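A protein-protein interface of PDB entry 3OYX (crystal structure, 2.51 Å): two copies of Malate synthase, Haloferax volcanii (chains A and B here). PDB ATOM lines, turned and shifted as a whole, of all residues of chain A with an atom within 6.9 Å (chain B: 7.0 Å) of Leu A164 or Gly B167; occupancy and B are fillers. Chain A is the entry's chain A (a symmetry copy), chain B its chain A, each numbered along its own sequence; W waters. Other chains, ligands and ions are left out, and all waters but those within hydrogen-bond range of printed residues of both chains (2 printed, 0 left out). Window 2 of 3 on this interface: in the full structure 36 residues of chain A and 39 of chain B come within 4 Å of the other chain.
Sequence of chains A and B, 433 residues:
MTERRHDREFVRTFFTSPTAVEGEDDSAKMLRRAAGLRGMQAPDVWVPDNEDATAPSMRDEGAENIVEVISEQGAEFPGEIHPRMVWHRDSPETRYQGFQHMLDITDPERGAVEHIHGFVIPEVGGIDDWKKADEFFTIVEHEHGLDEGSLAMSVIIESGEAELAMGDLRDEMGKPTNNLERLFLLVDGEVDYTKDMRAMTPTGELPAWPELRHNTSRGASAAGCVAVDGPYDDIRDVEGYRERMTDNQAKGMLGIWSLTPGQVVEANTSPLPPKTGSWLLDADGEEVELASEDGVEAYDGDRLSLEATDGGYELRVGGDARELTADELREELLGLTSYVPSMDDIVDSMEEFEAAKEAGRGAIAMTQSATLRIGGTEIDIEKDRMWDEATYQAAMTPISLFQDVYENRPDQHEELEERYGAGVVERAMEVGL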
ATOM      1  N   GLY A 125      -0.854 -21.938  17.679  1.00  0.00           N
ATOM      2  CA  GLY A 125      -2.044 -22.449  17.018  1.00  0.00           C
ATOM      3  C   GLY A 125      -2.862 -21.285  16.528  1.00  0.00           C
ATOM      4  O   GLY A 125      -2.329 -20.375  15.909  1.00  0.00           O
ATOM      5  N   GLY A 126      -4.143 -21.308  16.854  1.00  0.00           N
ATOM      6  CA  GLY A 126      -5.082 -20.244  16.507  1.00  0.00           C
ATOM      7  C   GLY A 126      -4.946 -19.029  17.415  1.00  0.00           C
ATOM      8  O   GLY A 126      -4.178 -19.071  18.414  1.00  0.00           O
ATOM      9  N   ILE A 127      -5.656 -17.928  17.087  1.00  0.00           N
ATOM     10  CA  ILE A 127      -5.409 -16.687  17.814  1.00  0.00           C
ATOM     11  C   ILE A 127      -5.503 -16.904  19.354  1.00  0.00           C
ATOM     12  O   ILE A 127      -4.766 -16.268  20.097  1.00  0.00           O
ATOM     13  CB  ILE A 127      -6.293 -15.556  17.311  1.00  0.00           C
ATOM     14  CG1 ILE A 127      -5.765 -14.203  17.796  1.00  0.00           C
ATOM     15  CG2 ILE A 127      -7.738 -15.768  17.742  1.00  0.00           C
ATOM     16  CD1 ILE A 127      -4.477 -13.841  17.018  1.00  0.00           C
ATOM     17  N   TRP A 130      -2.153 -17.655  20.596  1.00  0.00           N
ATOM     18  CA  TRP A 130      -1.247 -16.533  20.678  1.00  0.00           C
ATOM     19  C   TRP A 130      -1.519 -15.720  21.954  1.00  0.00           C
ATOM     20  O   TRP A 130      -0.591 -15.191  22.563  1.00  0.00           O
ATOM     21  CB  TRP A 130      -1.354 -15.591  19.461  1.00  0.00           C
ATOM     22  CG  TRP A 130      -1.167 -16.214  18.128  1.00  0.00           C
ATOM     23  CD1 TRP A 130      -1.454 -17.527  17.792  1.00  0.00           C
ATOM     24  CD2 TRP A 130      -0.730 -15.576  16.913  1.00  0.00           C
ATOM     25  NE1 TRP A 130      -1.197 -17.729  16.457  1.00  0.00           N
ATOM     26  CE2 TRP A 130      -0.776 -16.551  15.890  1.00  0.00           C
ATOM     27  CE3 TRP A 130      -0.296 -14.291  16.587  1.00  0.00           C
ATOM     28  CZ2 TRP A 130      -0.399 -16.275  14.571  1.00  0.00           C
ATOM     29  CZ3 TRP A 130       0.034 -13.987  15.230  1.00  0.00           C
ATOM     30  CH2 TRP A 130       0.003 -14.978  14.254  1.00  0.00           C
ATOM     31  N   ILE A 157       5.101 -19.296  12.245  1.00  0.00           N
ATOM     32  CA  ILE A 157       3.932 -19.824  11.600  1.00  0.00           C
ATOM     33  C   ILE A 157       4.241 -21.213  11.046  1.00  0.00           C
ATOM     34  O   ILE A 157       4.842 -21.362   9.962  1.00  0.00           O
ATOM     35  CB  ILE A 157       3.478 -18.906  10.481  1.00  0.00           C
ATOM     36  CG1 ILE A 157       3.358 -17.473  11.056  1.00  0.00           C
ATOM     37  CG2 ILE A 157       2.184 -19.538   9.804  1.00  0.00           C
ATOM     38  CD1 ILE A 157       2.075 -17.179  11.898  1.00  0.00           C
ATOM     39  N   SER A 159       1.925 -24.173  11.490  1.00  0.00           N
ATOM     40  CA  SER A 159       0.755 -25.023  11.393  1.00  0.00           C
ATOM     41  C   SER A 159      -0.307 -24.344  10.585  1.00  0.00           C
ATOM     42  O   SER A 159      -0.279 -23.101  10.446  1.00  0.00           O
ATOM     43  CB  SER A 159       0.212 -25.302  12.776  1.00  0.00           C
ATOM     44  OG  SER A 159      -0.195 -24.106  13.399  1.00  0.00           O
ATOM     45  N   GLY A 160      -1.262 -25.139  10.074  1.00  0.00           N
ATOM     46  CA  GLY A 160      -2.460 -24.615   9.383  1.00  0.00           C
ATOM     47  C   GLY A 160      -3.252 -23.634  10.249  1.00  0.00           C
ATOM     48  O   GLY A 160      -3.650 -22.573   9.743  1.00  0.00           O
ATOM     49  N   GLU A 161      -3.440 -23.923  11.547  1.00  0.00           N
ATOM     50  CA  GLU A 161      -4.234 -23.044  12.391  1.00  0.00           C
ATOM     51  C   GLU A 161      -3.549 -21.668  12.446  1.00  0.00           C
ATOM     52  O   GLU A 161      -4.248 -20.660  12.420  1.00  0.00           O
ATOM     53  CB  GLU A 161      -4.430 -23.548  13.830  1.00  0.00           C
ATOM     54  CG  GLU A 161      -4.707 -24.993  14.103  1.00  0.00           C
ATOM     55  CD  GLU A 161      -5.083 -25.292  15.601  1.00  0.00           C
ATOM     56  OE1 GLU A 161      -4.330 -26.069  16.246  1.00  0.00           O
ATOM     57  OE2 GLU A 161      -6.115 -24.773  16.166  1.00  0.00           O
ATOM     58  N   ALA A 162      -2.201 -21.618  12.523  1.00  0.00           N
ATOM     59  CA  ALA A 162      -1.507 -20.354  12.672  1.00  0.00           C
ATOM     60  C   ALA A 162      -1.589 -19.564  11.390  1.00  0.00           C
ATOM     61  O   ALA A 162      -1.696 -18.327  11.433  1.00  0.00           O
ATOM     62  CB  ALA A 162      -0.077 -20.601  13.022  1.00  0.00           C
ATOM     63  N   GLU A 163      -1.522 -20.252  10.247  1.00  0.00           N
ATOM     64  CA  GLU A 163      -1.678 -19.603   8.985  1.00  0.00           C
ATOM     65  C   GLU A 163      -3.047 -18.939   8.923  1.00  0.00           C
ATOM     66  O   GLU A 163      -3.165 -17.846   8.367  1.00  0.00           O
ATOM     67  CB  GLU A 163      -1.600 -20.615   7.852  1.00  0.00           C
ATOM     68  CG  GLU A 163      -1.619 -19.960   6.484  1.00  0.00           C
ATOM     69  CD  GLU A 163      -1.701 -20.994   5.388  1.00  0.00           C
ATOM     70  OE1 GLU A 163      -1.577 -22.190   5.755  1.00  0.00           O
ATOM     71  OE2 GLU A 163      -1.933 -20.636   4.196  1.00  0.00           O
ATOM     72  N   LEU A 164      -4.079 -19.600   9.447  1.00  0.00           N
ATOM     73  CA  LEU A 164      -5.424 -18.990   9.458  1.00  0.00           C
ATOM     74  C   LEU A 164      -5.518 -17.821  10.456  1.00  0.00           C
ATOM     75  O   LEU A 164      -6.200 -16.820  10.171  1.00  0.00           O
ATOM     76  CB  LEU A 164      -6.555 -20.017   9.712  1.00  0.00           C
ATOM     77  CG  LEU A 164      -6.773 -20.984   8.547  1.00  0.00           C
ATOM     78  CD1 LEU A 164      -7.504 -22.248   8.942  1.00  0.00           C
ATOM     79  CD2 LEU A 164      -7.400 -20.242   7.337  1.00  0.00           C
ATOM     80  N   ALA A 165      -4.785 -17.915  11.565  1.00  0.00           N
ATOM     81  CA  ALA A 165      -4.874 -16.956  12.656  1.00  0.00           C
ATOM     82  C   ALA A 165      -4.449 -15.589  12.213  1.00  0.00           C
ATOM     83  O   ALA A 165      -4.846 -14.607  12.794  1.00  0.00           O
ATOM     84  CB  ALA A 165      -4.066 -17.404  13.845  1.00  0.00           C
ATOM     85  N   MET A 166      -3.661 -15.504  11.153  1.00  0.00           N
ATOM     86  CA  MET A 166      -3.147 -14.211  10.694  1.00  0.00           C
ATOM     87  C   MET A 166      -4.223 -13.360  10.082  1.00  0.00           C
ATOM     88  O   MET A 166      -4.036 -12.176   9.956  1.00  0.00           O
ATOM     89  CB  MET A 166      -2.010 -14.356   9.682  1.00  0.00           C
ATOM     90  CG  MET A 166      -0.746 -14.758  10.299  1.00  0.00           C
ATOM     91  SD  MET A 166       0.574 -15.094   9.135  1.00  0.00           S
ATOM     92  CE  MET A 166      -0.057 -16.378   8.064  1.00  0.00           C
ATOM     93  N   GLY A 167      -5.357 -13.946   9.745  1.00  0.00           N
ATOM     94  CA  GLY A 167      -6.410 -13.239   9.020  1.00  0.00           C
ATOM     95  C   GLY A 167      -7.256 -12.237   9.790  1.00  0.00           C
ATOM     96  O   GLY A 167      -7.897 -11.405   9.175  1.00  0.00           O
ATOM     97  N   ASP A 168      -7.301 -12.294  11.119  1.00  0.00           N
ATOM     98  CA  ASP A 168      -8.124 -11.355  11.882  1.00  0.00           C
ATOM     99  C   ASP A 168      -7.275 -10.722  13.015  1.00  0.00           C
ATOM    100  O   ASP A 168      -7.770 -10.227  14.040  1.00  0.00           O
ATOM    101  CB  ASP A 168      -9.371 -12.068  12.419  1.00  0.00           C
ATOM    102  CG  ASP A 168     -10.427 -11.097  12.927  1.00  0.00           C
ATOM    103  OD1 ASP A 168     -10.498  -9.943  12.418  1.00  0.00           O
ATOM    104  OD2 ASP A 168     -11.184 -11.483  13.842  1.00  0.00           O
ATOM    105  N   LEU A 169      -5.977 -10.746  12.791  1.00  0.00           N
ATOM    106  CA  LEU A 169      -5.008 -10.273  13.715  1.00  0.00           C
ATOM    107  C   LEU A 169      -5.274  -8.824  14.061  1.00  0.00           C
ATOM    108  O   LEU A 169      -5.155  -8.464  15.228  1.00  0.00           O
ATOM    109  CB  LEU A 169      -3.668 -10.406  13.032  1.00  0.00           C
ATOM    110  CG  LEU A 169      -2.419 -10.578  13.843  1.00  0.00           C
ATOM    111  CD1 LEU A 169      -2.795 -11.333  15.111  1.00  0.00           C
ATOM    112  CD2 LEU A 169      -1.393 -11.325  13.009  1.00  0.00           C
ATOM    113  N   ALA B 162     -17.656 -22.105  -0.160  1.00  0.00           N
ATOM    114  CA  ALA B 162     -17.224 -23.263   0.594  1.00  0.00           C
ATOM    115  C   ALA B 162     -15.739 -23.185   0.855  1.00  0.00           C
ATOM    116  O   ALA B 162     -15.280 -23.602   1.932  1.00  0.00           O
ATOM    117  CB  ALA B 162     -17.537 -24.508  -0.167  1.00  0.00           C
ATOM    118  N   GLU B 163     -14.978 -22.675  -0.116  1.00  0.00           N
ATOM    119  CA  GLU B 163     -13.576 -22.480   0.071  1.00  0.00           C
ATOM    120  C   GLU B 163     -13.349 -21.530   1.239  1.00  0.00           C
ATOM    121  O   GLU B 163     -12.403 -21.727   2.005  1.00  0.00           O
ATOM    122  CB  GLU B 163     -12.955 -21.853  -1.167  1.00  0.00           C
ATOM    123  CG  GLU B 163     -11.444 -21.754  -1.074  1.00  0.00           C
ATOM    124  CD  GLU B 163     -10.879 -20.985  -2.244  1.00  0.00           C
ATOM    125  OE1 GLU B 163     -11.693 -20.704  -3.159  1.00  0.00           O
ATOM    126  OE2 GLU B 163      -9.664 -20.624  -2.236  1.00  0.00           O
ATOM    127  N   LEU B 164     -14.172 -20.489   1.359  1.00  0.00           N
ATOM    128  CA  LEU B 164     -14.031 -19.557   2.495  1.00  0.00           C
ATOM    129  C   LEU B 164     -14.466 -20.199   3.825  1.00  0.00           C
ATOM    130  O   LEU B 164     -13.848 -19.933   4.871  1.00  0.00           O
ATOM    131  CB  LEU B 164     -14.767 -18.213   2.273  1.00  0.00           C
ATOM    132  CG  LEU B 164     -14.120 -17.335   1.200  1.00  0.00           C
ATOM    133  CD1 LEU B 164     -15.051 -16.281   0.643  1.00  0.00           C
ATOM    134  CD2 LEU B 164     -12.762 -16.777   1.703  1.00  0.00           C
ATOM    135  N   ALA B 165     -15.458 -21.087   3.769  1.00  0.00           N
ATOM    136  CA  ALA B 165     -16.064 -21.674   4.955  1.00  0.00           C
ATOM    137  C   ALA B 165     -15.069 -22.488   5.727  1.00  0.00           C
ATOM    138  O   ALA B 165     -15.224 -22.683   6.909  1.00  0.00           O
ATOM    139  CB  ALA B 165     -17.269 -22.504   4.601  1.00  0.00           C
ATOM    140  N   MET B 166     -14.012 -22.945   5.074  1.00  0.00           N
ATOM    141  CA  MET B 166     -13.028 -23.803   5.737  1.00  0.00           C
ATOM    142  C   MET B 166     -12.201 -23.047   6.737  1.00  0.00           C
ATOM    143  O   MET B 166     -11.588 -23.657   7.576  1.00  0.00           O
ATOM    144  CB  MET B 166     -12.083 -24.486   4.748  1.00  0.00           C
ATOM    145  CG  MET B 166     -12.715 -25.592   4.027  1.00  0.00           C
ATOM    146  SD  MET B 166     -11.698 -26.321   2.745  1.00  0.00           S
ATOM    147  CE  MET B 166     -11.297 -24.975   1.639  1.00  0.00           C
ATOM    148  N   GLY B 167     -12.220 -21.728   6.682  1.00  0.00           N
ATOM    149  CA  GLY B 167     -11.348 -20.904   7.518  1.00  0.00           C
ATOM    150  C   GLY B 167     -11.699 -20.761   8.990  1.00  0.00           C
ATOM    151  O   GLY B 167     -10.847 -20.379   9.769  1.00  0.00           O
ATOM    152  N   ASP B 168     -12.935 -21.037   9.403  1.00  0.00           N
ATOM    153  CA  ASP B 168     -13.304 -20.886  10.811  1.00  0.00           C
ATOM    154  C   ASP B 168     -14.011 -22.175  11.303  1.00  0.00           C
ATOM    155  O   ASP B 168     -14.777 -22.200  12.280  1.00  0.00           O
ATOM    156  CB  ASP B 168     -14.177 -19.639  10.994  1.00  0.00           C
ATOM    157  CG  ASP B 168     -14.319 -19.232  12.453  1.00  0.00           C
ATOM    158  OD1 ASP B 168     -13.387 -19.507  13.263  1.00  0.00           O
ATOM    159  OD2 ASP B 168     -15.365 -18.642  12.797  1.00  0.00           O
ATOM    160  N   LEU B 169     -13.722 -23.250  10.597  1.00  0.00           N
ATOM    161  CA  LEU B 169     -14.297 -24.526  10.832  1.00  0.00           C
ATOM    162  C   LEU B 169     -14.036 -24.967  12.257  1.00  0.00           C
ATOM    163  O   LEU B 169     -14.942 -25.513  12.881  1.00  0.00           O
ATOM    164  CB  LEU B 169     -13.631 -25.477   9.867  1.00  0.00           C
ATOM    165  CG  LEU B 169     -14.347 -26.711   9.405  1.00  0.00           C
ATOM    166  CD1 LEU B 169     -15.837 -26.396   9.383  1.00  0.00           C
ATOM    167  CD2 LEU B 169     -13.819 -27.099   8.034  1.00  0.00           C
ATOM    168  N   ARG B 170     -12.825 -24.744  12.770  1.00  0.00           N
ATOM    169  CA  ARG B 170     -12.430 -25.244  14.095  1.00  0.00           C
ATOM    170  C   ARG B 170     -13.410 -24.750  15.149  1.00  0.00           C
ATOM    171  O   ARG B 170     -13.949 -25.509  15.921  1.00  0.00           O
ATOM    172  CB  ARG B 170     -11.030 -24.756  14.452  1.00  0.00           C
ATOM    173  CG  ARG B 170     -10.307 -25.572  15.541  1.00  0.00           C
ATOM    174  CD  ARG B 170      -9.162 -24.746  16.249  1.00  0.00           C
ATOM    175  NE  ARG B 170      -9.552 -23.327  16.361  1.00  0.00           N
ATOM    176  CZ  ARG B 170      -8.849 -22.309  15.884  1.00  0.00           C
ATOM    177  NH1 ARG B 170      -7.679 -22.586  15.342  1.00  0.00           N
ATOM    178  NH2 ARG B 170      -9.331 -21.051  15.936  1.00  0.00           N
ATOM    179  N   ASP B 171     -13.709 -23.469  15.151  1.00  0.00           N
ATOM    180  CA  ASP B 171     -14.602 -22.916  16.141  1.00  0.00           C
ATOM    181  C   ASP B 171     -16.137 -23.125  15.846  1.00  0.00           C
ATOM    182  O   ASP B 171     -16.930 -23.197  16.769  1.00  0.00           O
ATOM    183  CB  ASP B 171     -14.259 -21.444  16.236  1.00  0.00           C
ATOM    184  CG  ASP B 171     -12.898 -21.183  16.921  1.00  0.00           C
ATOM    185  OD1 ASP B 171     -12.223 -22.100  17.459  1.00  0.00           O
ATOM    186  OD2 ASP B 171     -12.510 -19.994  16.934  1.00  0.00           O
ATOM    187  N   ASN B 215      -5.656 -24.335   0.071  1.00  0.00           N
ATOM    188  CA  ASN B 215      -6.644 -23.941   1.077  1.00  0.00           C
ATOM    189  C   ASN B 215      -7.377 -25.132   1.685  1.00  0.00           C
ATOM    190  O   ASN B 215      -7.762 -25.106   2.860  1.00  0.00           O
ATOM    191  CB  ASN B 215      -7.551 -22.858   0.471  1.00  0.00           C
ATOM    192  CG  ASN B 215      -6.778 -21.549   0.182  1.00  0.00           C
ATOM    193  OD1 ASN B 215      -5.688 -21.304   0.738  1.00  0.00           O
ATOM    194  ND2 ASN B 215      -7.336 -20.703  -0.676  1.00  0.00           N
ATOM    195  N   ARG B 218      -4.810 -27.009   3.982  1.00  0.00           N
ATOM    196  CA  ARG B 218      -4.843 -26.190   5.215  1.00  0.00           C
ATOM    197  C   ARG B 218      -6.098 -26.324   6.092  1.00  0.00           C
ATOM    198  O   ARG B 218      -6.019 -26.533   7.310  1.00  0.00           O
ATOM    199  CB  ARG B 218      -4.748 -24.738   4.813  1.00  0.00           C
ATOM    200  CG  ARG B 218      -4.855 -23.789   5.957  1.00  0.00           C
ATOM    201  CD  ARG B 218      -4.599 -22.452   5.336  1.00  0.00           C
ATOM    202  NE  ARG B 218      -5.806 -21.969   4.694  1.00  0.00           N
ATOM    203  CZ  ARG B 218      -5.883 -20.879   3.925  1.00  0.00           C
ATOM    204  NH1 ARG B 218      -4.789 -20.181   3.701  1.00  0.00           N
ATOM    205  NH2 ARG B 218      -7.061 -20.476   3.430  1.00  0.00           N
ATOM    206  N   GLY B 219      -7.272 -26.186   5.470  1.00  0.00           N
ATOM    207  CA  GLY B 219      -8.539 -26.342   6.186  1.00  0.00           C
ATOM    208  C   GLY B 219      -8.608 -27.695   6.858  1.00  0.00           C
ATOM    209  O   GLY B 219      -9.082 -27.829   8.008  1.00  0.00           O
ATOM    210  N   ALA B 222      -6.111 -27.750   9.880  1.00  0.00           N
ATOM    211  CA  ALA B 222      -6.646 -27.026  11.052  1.00  0.00           C
ATOM    212  C   ALA B 222      -7.873 -27.630  11.726  1.00  0.00           C
ATOM    213  O   ALA B 222      -8.235 -27.241  12.837  1.00  0.00           O
ATOM    214  CB  ALA B 222      -6.958 -25.595  10.675  1.00  0.00           C
ATOM    215  N   ALA B 223      -8.555 -28.572  11.096  1.00  0.00           N
ATOM    216  CA  ALA B 223      -9.902 -28.863  11.587  1.00  0.00           C
ATOM    217  C   ALA B 223      -9.971 -30.316  11.863  1.00  0.00           C
ATOM    218  O   ALA B 223     -11.005 -30.817  12.245  1.00  0.00           O
ATOM    219  CB  ALA B 223     -10.942 -28.476  10.571  1.00  0.00           C
HETATM  220  O   HOH W   1      -6.889 -20.661  13.312  1.00  0.00           O
HETATM  221  O   HOH W   2      -8.001 -19.705  18.427  1.00  0.00           O
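NH1 of Arg B170 lies within salt-bridge range of OE2 of Glu A161 (2.8 Å).
The guanidinium group (NH1) of Arg B218 lies within salt-bridge range of the side-chain carboxylate (OE2) of Glu A163 (2.9 Å).
NE of Arg B170 lies within salt-bridge range of OD1 of Asp B171 (3.1 Å).
The side-chain amide oxygen (OD1) of Asn B215 lies within hydrogen-bond range of the guanidinium group (NH2) of Arg B218 (3.1 Å).
Among the printed residues, merely in contact across the chains: Leu A164 with Arg B218 (3.5 Å), Gly A126 with Arg B170 (3.7 Å), Leu A164 with Ala B222 (3.8 Å), Leu A164 with Gly B167 (3.9 Å) and Glu A161 with Ala B222 (3.99 Å).
Of chain B, only Gly B167 (3.9 Å), Arg B218 (3.5 Å) and Ala B222 (3.8 Å) come within 4 Å of Leu A164.
Gly B167 touches just one residue of chain A: Leu A164.
Printed residues of chain A within 4 Å of Arg B170: Gly A126 (3.7 Å) and Glu A161 (2.8 Å).
Of the printed residues of chain A, Arg B218 touches Glu A163 (2.9 Å) and Leu A164 (3.5 Å).
The nearest residue of chain A that does not touch Gly B167 is Ala A165 (6.8 Å).
Leu A164 touches Gly B167, but with the chains exchanged Gly A167 does not touch Leu B164 (10.3 Å).
8 positions are printed for both chains.
Of the 7 pairs that touch across the chains among the printed residues, none has its exchanged pair printed and touching as well.
Water W1 lies within hydrogen-bond range of O of Glu A161 (2.8 Å) and NH1 of Arg B170 (2.9 Å).
Water W2 bridges the guanidinium group of Arg B170 and the backbone NH of Ile A127.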
